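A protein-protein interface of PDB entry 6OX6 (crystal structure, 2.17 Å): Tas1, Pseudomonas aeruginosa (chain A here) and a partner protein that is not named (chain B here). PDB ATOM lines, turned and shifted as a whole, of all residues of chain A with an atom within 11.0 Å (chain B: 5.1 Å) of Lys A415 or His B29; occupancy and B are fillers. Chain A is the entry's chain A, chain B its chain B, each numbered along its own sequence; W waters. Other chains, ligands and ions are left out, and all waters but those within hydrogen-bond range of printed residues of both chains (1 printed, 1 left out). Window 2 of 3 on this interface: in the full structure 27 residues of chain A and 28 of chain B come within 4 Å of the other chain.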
ATOM      1  N   TRP A 409     -22.012  20.076 -15.107  1.00  0.00           N
ATOM      2  CA  TRP A 409     -21.224  19.221 -15.988  1.00  0.00           C
ATOM      3  C   TRP A 409     -19.785  19.117 -15.512  1.00  0.00           C
ATOM      4  O   TRP A 409     -19.200  18.026 -15.529  1.00  0.00           O
ATOM      5  CB  TRP A 409     -21.279  19.767 -17.417  1.00  0.00           C
ATOM      6  CG  TRP A 409     -20.597  18.930 -18.452  1.00  0.00           C
ATOM      7  CD1 TRP A 409     -21.127  17.846 -19.125  1.00  0.00           C
ATOM      8  CD2 TRP A 409     -19.267  19.111 -18.969  1.00  0.00           C
ATOM      9  NE1 TRP A 409     -20.205  17.370 -20.038  1.00  0.00           N
ATOM     10  CE2 TRP A 409     -19.061  18.119 -19.953  1.00  0.00           C
ATOM     11  CE3 TRP A 409     -18.236  20.024 -18.700  1.00  0.00           C
ATOM     12  CZ2 TRP A 409     -17.875  18.005 -20.655  1.00  0.00           C
ATOM     13  CZ3 TRP A 409     -17.056  19.908 -19.407  1.00  0.00           C
ATOM     14  CH2 TRP A 409     -16.880  18.906 -20.365  1.00  0.00           C
ATOM     15  N   ARG A 410     -19.230  20.239 -15.025  1.00  0.00           N
ATOM     16  CA  ARG A 410     -17.823  20.306 -14.676  1.00  0.00           C
ATOM     17  C   ARG A 410     -17.476  19.367 -13.535  1.00  0.00           C
ATOM     18  O   ARG A 410     -16.388  18.772 -13.528  1.00  0.00           O
ATOM     19  CB  ARG A 410     -17.468  21.736 -14.304  1.00  0.00           C
ATOM     20  CG  ARG A 410     -16.138  21.889 -13.604  1.00  0.00           C
ATOM     21  CD  ARG A 410     -15.827  23.344 -13.326  1.00  0.00           C
ATOM     22  NE  ARG A 410     -14.706  23.462 -12.400  1.00  0.00           N
ATOM     23  CZ  ARG A 410     -14.068  24.606 -12.122  1.00  0.00           C
ATOM     24  NH1 ARG A 410     -14.435  25.745 -12.721  1.00  0.00           N
ATOM     25  NH2 ARG A 410     -13.063  24.616 -11.248  1.00  0.00           N
ATOM     26  N   VAL A 411     -18.354  19.252 -12.525  1.00  0.00           N
ATOM     27  CA  VAL A 411     -18.007  18.396 -11.389  1.00  0.00           C
ATOM     28  C   VAL A 411     -18.107  16.904 -11.699  1.00  0.00           C
ATOM     29  O   VAL A 411     -17.764  16.082 -10.851  1.00  0.00           O
ATOM     30  CB  VAL A 411     -18.878  18.714 -10.156  1.00  0.00           C
ATOM     31  CG1 VAL A 411     -18.671  20.166  -9.730  1.00  0.00           C
ATOM     32  CG2 VAL A 411     -20.338  18.459 -10.457  1.00  0.00           C
ATOM     33  N   LEU A 412     -18.579  16.514 -12.877  1.00  0.00           N
ATOM     34  CA  LEU A 412     -18.759  15.088 -13.159  1.00  0.00           C
ATOM     35  C   LEU A 412     -17.424  14.426 -13.465  1.00  0.00           C
ATOM     36  O   LEU A 412     -16.542  15.027 -14.089  1.00  0.00           O
ATOM     37  CB  LEU A 412     -19.722  14.901 -14.340  1.00  0.00           C
ATOM     38  CG  LEU A 412     -21.137  15.453 -14.063  1.00  0.00           C
ATOM     39  CD1 LEU A 412     -22.004  15.417 -15.333  1.00  0.00           C
ATOM     40  CD2 LEU A 412     -21.827  14.700 -12.894  1.00  0.00           C
ATOM     41  N   ASP A 413     -17.281  13.183 -13.018  1.00  0.00           N
ATOM     42  CA  ASP A 413     -16.139  12.353 -13.378  1.00  0.00           C
ATOM     43  C   ASP A 413     -16.129  12.153 -14.896  1.00  0.00           C
ATOM     44  O   ASP A 413     -17.188  12.216 -15.532  1.00  0.00           O
ATOM     45  CB  ASP A 413     -16.246  11.017 -12.622  1.00  0.00           C
ATOM     46  CG  ASP A 413     -15.268   9.963 -13.107  1.00  0.00           C
ATOM     47  OD1 ASP A 413     -14.256   9.715 -12.414  1.00  0.00           O
ATOM     48  OD2 ASP A 413     -15.503   9.377 -14.182  1.00  0.00           O
ATOM     49  N   PRO A 414     -14.957  11.932 -15.511  1.00  0.00           N
ATOM     50  CA  PRO A 414     -14.910  11.883 -16.982  1.00  0.00           C
ATOM     51  C   PRO A 414     -15.696  10.709 -17.582  1.00  0.00           C
ATOM     52  O   PRO A 414     -16.106  10.788 -18.746  1.00  0.00           O
ATOM     53  CB  PRO A 414     -13.410  11.778 -17.294  1.00  0.00           C
ATOM     54  CG  PRO A 414     -12.717  12.354 -16.069  1.00  0.00           C
ATOM     55  CD  PRO A 414     -13.597  11.956 -14.913  1.00  0.00           C
ATOM     56  N   LYS A 415     -15.955   9.650 -16.817  1.00  0.00           N
ATOM     57  CA  LYS A 415     -16.778   8.554 -17.302  1.00  0.00           C
ATOM     58  C   LYS A 415     -18.194   8.595 -16.733  1.00  0.00           C
ATOM     59  O   LYS A 415     -18.881   7.568 -16.733  1.00  0.00           O
ATOM     60  CB  LYS A 415     -16.104   7.196 -17.021  1.00  0.00           C
ATOM     61  CG  LYS A 415     -15.809   6.907 -15.582  1.00  0.00           C
ATOM     62  CD  LYS A 415     -15.042   5.585 -15.319  1.00  0.00           C
ATOM     63  CE  LYS A 415     -13.770   5.434 -16.135  1.00  0.00           C
ATOM     64  NZ  LYS A 415     -12.965   4.233 -15.685  1.00  0.00           N
ATOM     65  N   SER A 416     -18.670   9.767 -16.292  1.00  0.00           N
ATOM     66  CA  SER A 416     -19.983   9.815 -15.644  1.00  0.00           C
ATOM     67  C   SER A 416     -21.116   9.425 -16.601  1.00  0.00           C
ATOM     68  O   SER A 416     -21.159   9.886 -17.749  1.00  0.00           O
ATOM     69  CB  SER A 416     -20.264  11.208 -15.080  1.00  0.00           C
ATOM     70  OG  SER A 416     -21.676  11.341 -14.877  1.00  0.00           O
ATOM     71  N   PRO A 417     -22.075   8.615 -16.143  1.00  0.00           N
ATOM     72  CA  PRO A 417     -23.304   8.386 -16.931  1.00  0.00           C
ATOM     73  C   PRO A 417     -24.187   9.621 -17.107  1.00  0.00           C
ATOM     74  O   PRO A 417     -25.094   9.603 -17.960  1.00  0.00           O
ATOM     75  CB  PRO A 417     -24.046   7.308 -16.125  1.00  0.00           C
ATOM     76  CG  PRO A 417     -22.988   6.657 -15.279  1.00  0.00           C
ATOM     77  CD  PRO A 417     -22.009   7.751 -14.946  1.00  0.00           C
ATOM     78  N   GLU A 418     -23.983  10.626 -16.256  1.00  0.00           N
ATOM     79  CA  GLU A 418     -24.779  11.855 -16.277  1.00  0.00           C
ATOM     80  C   GLU A 418     -24.333  12.953 -17.251  1.00  0.00           C
ATOM     81  O   GLU A 418     -25.162  13.747 -17.694  1.00  0.00           O
ATOM     82  CB  GLU A 418     -24.974  12.374 -14.848  1.00  0.00           C
ATOM     83  CG  GLU A 418     -25.480  11.328 -13.870  1.00  0.00           C
ATOM     84  CD  GLU A 418     -25.609  11.863 -12.457  1.00  0.00           C
ATOM     85  OE1 GLU A 418     -24.673  11.661 -11.656  1.00  0.00           O
ATOM     86  OE2 GLU A 418     -26.647  12.486 -12.149  1.00  0.00           O
ATOM     87  N   ALA A 419     -23.049  13.012 -17.592  1.00  0.00           N
ATOM     88  CA  ALA A 419     -22.597  14.049 -18.527  1.00  0.00           C
ATOM     89  C   ALA A 419     -23.377  14.296 -19.812  1.00  0.00           C
ATOM     90  O   ALA A 419     -23.728  15.432 -20.131  1.00  0.00           O
ATOM     91  CB  ALA A 419     -21.116  13.832 -18.842  1.00  0.00           C
ATOM     92  N   GLN A 420     -23.658  13.239 -20.555  1.00  0.00           N
ATOM     93  CA  GLN A 420     -24.245  13.404 -21.877  1.00  0.00           C
ATOM     94  C   GLN A 420     -25.599  14.115 -21.812  1.00  0.00           C
ATOM     95  O   GLN A 420     -25.891  14.990 -22.637  1.00  0.00           O
ATOM     96  CB  GLN A 420     -24.349  12.033 -22.527  1.00  0.00           C
ATOM     97  CG  GLN A 420     -24.631  12.061 -23.988  1.00  0.00           C
ATOM     98  CD  GLN A 420     -26.004  11.546 -24.260  1.00  0.00           C
ATOM     99  OE1 GLN A 420     -26.230  10.332 -24.277  1.00  0.00           O
ATOM    100  NE2 GLN A 420     -26.953  12.468 -24.442  1.00  0.00           N
ATOM    101  N   ALA A 421     -26.432  13.786 -20.814  1.00  0.00           N
ATOM    102  CA  ALA A 421     -27.743  14.436 -20.720  1.00  0.00           C
ATOM    103  C   ALA A 421     -27.623  15.916 -20.361  1.00  0.00           C
ATOM    104  O   ALA A 421     -28.412  16.742 -20.838  1.00  0.00           O
ATOM    105  CB  ALA A 421     -28.630  13.730 -19.694  1.00  0.00           C
ATOM    106  N   GLY B   6     -17.925  10.664 -20.612  1.00  0.00           N
ATOM    107  CA  GLY B   6     -18.720   9.463 -20.817  1.00  0.00           C
ATOM    108  C   GLY B   6     -18.016   8.317 -21.526  1.00  0.00           C
ATOM    109  O   GLY B   6     -16.957   7.854 -21.083  1.00  0.00           O
ATOM    110  N   PHE B   9     -13.992   7.714 -22.152  1.00  0.00           N
ATOM    111  CA  PHE B   9     -13.163   7.629 -20.960  1.00  0.00           C
ATOM    112  C   PHE B   9     -13.322   6.297 -20.243  1.00  0.00           C
ATOM    113  O   PHE B   9     -12.427   5.868 -19.505  1.00  0.00           O
ATOM    114  CB  PHE B   9     -13.527   8.781 -20.023  1.00  0.00           C
ATOM    115  CG  PHE B   9     -13.035  10.107 -20.508  1.00  0.00           C
ATOM    116  CD1 PHE B   9     -13.820  10.888 -21.341  1.00  0.00           C
ATOM    117  CD2 PHE B   9     -11.764  10.543 -20.176  1.00  0.00           C
ATOM    118  CE1 PHE B   9     -13.353  12.106 -21.812  1.00  0.00           C
ATOM    119  CE2 PHE B   9     -11.287  11.763 -20.637  1.00  0.00           C
ATOM    120  CZ  PHE B   9     -12.089  12.546 -21.464  1.00  0.00           C
ATOM    121  N   ALA B  10     -14.466   5.661 -20.388  1.00  0.00           N
ATOM    122  CA  ALA B  10     -14.608   4.345 -19.800  1.00  0.00           C
ATOM    123  C   ALA B  10     -14.103   3.253 -20.723  1.00  0.00           C
ATOM    124  O   ALA B  10     -13.792   2.163 -20.240  1.00  0.00           O
ATOM    125  CB  ALA B  10     -16.062   4.075 -19.424  1.00  0.00           C
ATOM    126  N   ARG B  11     -14.104   3.531 -22.023  1.00  0.00           N
ATOM    127  CA  ARG B  11     -13.588   2.632 -23.056  1.00  0.00           C
ATOM    128  C   ARG B  11     -12.060   2.410 -23.109  1.00  0.00           C
ATOM    129  O   ARG B  11     -11.602   1.288 -23.330  1.00  0.00           O
ATOM    130  CB  ARG B  11     -14.088   3.074 -24.435  1.00  0.00           C
ATOM    131  CG  ARG B  11     -15.466   2.544 -24.795  1.00  0.00           C
ATOM    132  CD  ARG B  11     -15.545   2.164 -26.265  1.00  0.00           C
ATOM    133  NE  ARG B  11     -14.908   3.159 -27.121  1.00  0.00           N
ATOM    134  CZ  ARG B  11     -15.431   4.349 -27.402  1.00  0.00           C
ATOM    135  NH1 ARG B  11     -16.605   4.697 -26.892  1.00  0.00           N
ATOM    136  NH2 ARG B  11     -14.780   5.192 -28.192  1.00  0.00           N
ATOM    137  N   ARG B  12     -11.280   3.476 -22.910  1.00  0.00           N
ATOM    138  CA  ARG B  12      -9.833   3.408 -23.034  1.00  0.00           C
ATOM    139  C   ARG B  12      -9.092   4.654 -22.581  1.00  0.00           C
ATOM    140  O   ARG B  12      -9.699   5.671 -22.273  1.00  0.00           O
ATOM    141  CB  ARG B  12      -9.519   3.307 -24.530  1.00  0.00           C
ATOM    142  CG  ARG B  12      -9.946   4.564 -25.280  1.00  0.00           C
ATOM    143  CD  ARG B  12     -10.099   4.381 -26.781  1.00  0.00           C
ATOM    144  NE  ARG B  12     -11.008   5.377 -27.339  1.00  0.00           N
ATOM    145  CZ  ARG B  12     -10.642   6.600 -27.709  1.00  0.00           C
ATOM    146  NH1 ARG B  12      -9.383   6.979 -27.593  1.00  0.00           N
ATOM    147  NH2 ARG B  12     -11.536   7.444 -28.197  1.00  0.00           N
ATOM    148  N   ASP B  13      -7.767   4.547 -22.529  1.00  0.00           N
ATOM    149  CA  ASP B  13      -6.920   5.698 -22.301  1.00  0.00           C
ATOM    150  C   ASP B  13      -7.211   6.789 -23.324  1.00  0.00           C
ATOM    151  O   ASP B  13      -7.506   6.514 -24.488  1.00  0.00           O
ATOM    152  CB  ASP B  13      -5.451   5.287 -22.370  1.00  0.00           C
ATOM    153  CG  ASP B  13      -5.032   4.375 -21.210  1.00  0.00           C
ATOM    154  OD1 ASP B  13      -5.880   4.003 -20.363  1.00  0.00           O
ATOM    155  OD2 ASP B  13      -3.824   4.078 -21.122  1.00  0.00           O
ATOM    156  N   TRP B  27      -5.309  10.514 -19.625  1.00  0.00           N
ATOM    157  CA  TRP B  27      -6.295   9.790 -18.838  1.00  0.00           C
ATOM    158  C   TRP B  27      -5.978   8.297 -18.862  1.00  0.00           C
ATOM    159  O   TRP B  27      -5.760   7.710 -19.925  1.00  0.00           O
ATOM    160  CB  TRP B  27      -7.694  10.078 -19.382  1.00  0.00           C
ATOM    161  CG  TRP B  27      -8.794   9.133 -18.980  1.00  0.00           C
ATOM    162  CD1 TRP B  27      -9.357   8.157 -19.753  1.00  0.00           C
ATOM    163  CD2 TRP B  27      -9.487   9.092 -17.715  1.00  0.00           C
ATOM    164  NE1 TRP B  27     -10.347   7.507 -19.050  1.00  0.00           N
ATOM    165  CE2 TRP B  27     -10.443   8.060 -17.796  1.00  0.00           C
ATOM    166  CE3 TRP B  27      -9.381   9.824 -16.520  1.00  0.00           C
ATOM    167  CZ2 TRP B  27     -11.298   7.748 -16.737  1.00  0.00           C
ATOM    168  CZ3 TRP B  27     -10.228   9.513 -15.463  1.00  0.00           C
ATOM    169  CH2 TRP B  27     -11.180   8.484 -15.584  1.00  0.00           C
ATOM    170  N   ASP B  28      -5.944   7.691 -17.697  1.00  0.00           N
ATOM    171  CA  ASP B  28      -5.729   6.259 -17.538  1.00  0.00           C
ATOM    172  C   ASP B  28      -7.065   5.679 -17.089  1.00  0.00           C
ATOM    173  O   ASP B  28      -7.505   5.927 -15.962  1.00  0.00           O
ATOM    174  CB  ASP B  28      -4.613   6.014 -16.516  1.00  0.00           C
ATOM    175  CG  ASP B  28      -4.297   4.534 -16.299  1.00  0.00           C
ATOM    176  OD1 ASP B  28      -5.158   3.655 -16.531  1.00  0.00           O
ATOM    177  OD2 ASP B  28      -3.175   4.263 -15.840  1.00  0.00           O
ATOM    178  N   HIS B  29      -7.738   4.937 -17.969  1.00  0.00           N
ATOM    179  CA  HIS B  29      -9.092   4.531 -17.609  1.00  0.00           C
ATOM    180  C   HIS B  29      -9.085   3.471 -16.502  1.00  0.00           C
ATOM    181  O   HIS B  29      -9.945   3.503 -15.617  1.00  0.00           O
ATOM    182  CB  HIS B  29      -9.861   4.068 -18.848  1.00  0.00           C
ATOM    183  CG  HIS B  29      -9.546   2.673 -19.278  1.00  0.00           C
ATOM    184  ND1 HIS B  29      -8.468   2.367 -20.079  1.00  0.00           N
ATOM    185  CD2 HIS B  29     -10.173   1.501 -19.024  1.00  0.00           C
ATOM    186  CE1 HIS B  29      -8.440   1.064 -20.298  1.00  0.00           C
ATOM    187  NE2 HIS B  29      -9.471   0.517 -19.678  1.00  0.00           N
ATOM    188  N   ARG B  30      -8.105   2.564 -16.501  1.00  0.00           N
ATOM    189  CA  ARG B  30      -8.019   1.568 -15.434  1.00  0.00           C
ATOM    190  C   ARG B  30      -7.850   2.223 -14.064  1.00  0.00           C
ATOM    191  O   ARG B  30      -8.606   1.939 -13.130  1.00  0.00           O
ATOM    192  CB  ARG B  30      -6.875   0.601 -15.709  1.00  0.00           C
ATOM    193  CG  ARG B  30      -7.131  -0.324 -16.897  1.00  0.00           C
ATOM    194  CD  ARG B  30      -5.969  -1.316 -17.078  1.00  0.00           C
ATOM    195  NE  ARG B  30      -6.044  -2.483 -16.182  1.00  0.00           N
ATOM    196  CZ  ARG B  30      -5.484  -2.564 -14.968  1.00  0.00           C
ATOM    197  NH1 ARG B  30      -4.802  -1.537 -14.467  1.00  0.00           N
ATOM    198  NH2 ARG B  30      -5.602  -3.679 -14.246  1.00  0.00           N
ATOM    199  N   GLN B  31      -6.869   3.108 -13.920  1.00  0.00           N
ATOM    200  CA  GLN B  31      -6.670   3.736 -12.619  1.00  0.00           C
ATOM    201  C   GLN B  31      -7.655   4.862 -12.351  1.00  0.00           C
ATOM    202  O   GLN B  31      -7.816   5.260 -11.188  1.00  0.00           O
ATOM    203  CB  GLN B  31      -5.238   4.259 -12.487  1.00  0.00           C
ATOM    204  CG  GLN B  31      -4.184   3.172 -12.662  1.00  0.00           C
ATOM    205  CD  GLN B  31      -4.409   1.993 -11.731  1.00  0.00           C
ATOM    206  OE1 GLN B  31      -4.599   2.172 -10.524  1.00  0.00           O
ATOM    207  NE2 GLN B  31      -4.388   0.778 -12.288  1.00  0.00           N
ATOM    208  N   GLY B  32      -8.297   5.393 -13.389  1.00  0.00           N
ATOM    209  CA  GLY B  32      -9.200   6.521 -13.224  1.00  0.00           C
ATOM    210  C   GLY B  32      -8.501   7.839 -12.955  1.00  0.00           C
ATOM    211  O   GLY B  32      -9.060   8.704 -12.258  1.00  0.00           O
HETATM  212  O   HOH W   1     -13.058   2.262 -17.649  1.00  0.00           O
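Hydrophobic or aromatic side chains of chain A that line the printed part of chain B: Pro A414. Hydrophobic or aromatic side chains of chain B within 4 Å of the printed part of chain A: Phe B9, Ala B10 and Trp B27. Among the printed residues, no Asp or Glu carboxylate lies within 4 Å of a Lys or Arg side-chain nitrogen of the other chain.
Water W1 bridges O of Ala B10 and NZ of Lys A415.
The backbone carbonyl oxygen of Pro A414 lies within hydrogen-bond range of the backbone NH of Gly B6 (2.6 Å). The side-chain amino group (NZ) of Lys A415 sits at hydrogen-bond distance from the backbone carbonyl oxygen (O) of His B29 (3.1 Å).
Among the printed residues, pairs that only touch across the chains: Pro A414 with Phe B9, Pro A414 with Trp B27, Lys A415 with Gly B6, Lys A415 with Phe B9, Lys A415 with Ala B10, Lys A415 with Trp B27 and Ser A416 with Gly B6.
The backbone NH (N) of Lys A415 is in hydrogen-bond range of the side-chain carboxylate (OD2) of Asp A413 (2.7 Å). N of Glu A418 sits at hydrogen-bond distance from OG of Ser A416 (2.8 Å). The side-chain hydroxyl of Ser A416 sits at hydrogen-bond distance from the backbone NH of Ala A419 (3.5 Å). O of Phe B9 sits at hydrogen-bond distance from NE1 of Trp B27 (2.7 Å). OD1 of Asp B13 is in hydrogen-bond range of ND1 of His B29 (3.1 Å).
Lys A415 touches just these residues of chain B: Gly B6, Phe B9, Ala B10, Trp B27 and His B29. Of chain A, only Lys A415 (3.1 Å) comes within 4 Å of His B29. Of chain A, only Pro A414 (2.6 Å), Lys A415 (3.8 Å) and Ser A416 (3.9 Å) come within 4 Å of Gly B6. Phe B9 touches just these residues of chain A: Pro A414 (3.5 Å) and Lys A415 (3.7 Å). Ala B10 touches just one residue of chain A: Lys A415 (3.9 Å). No residue of chain A comes within 4 Å of Asp B13. No residue of chain A comes within 4 Å of Asp B28. No residue of chain A comes within 4 Å of Gly B32. Printed residues of chain B within 4 Å of Ser A416: Gly B6. Of the printed residues of chain B, Pro A414 touches Gly B6 (2.6 Å), Phe B9 (3.5 Å) and Trp B27 (3.8 Å). Trp A409 touches none of the printed residues of chain B. The nearest printed residue of chain B that does not touch Ser A416 is Phe B9 (6.4 Å).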
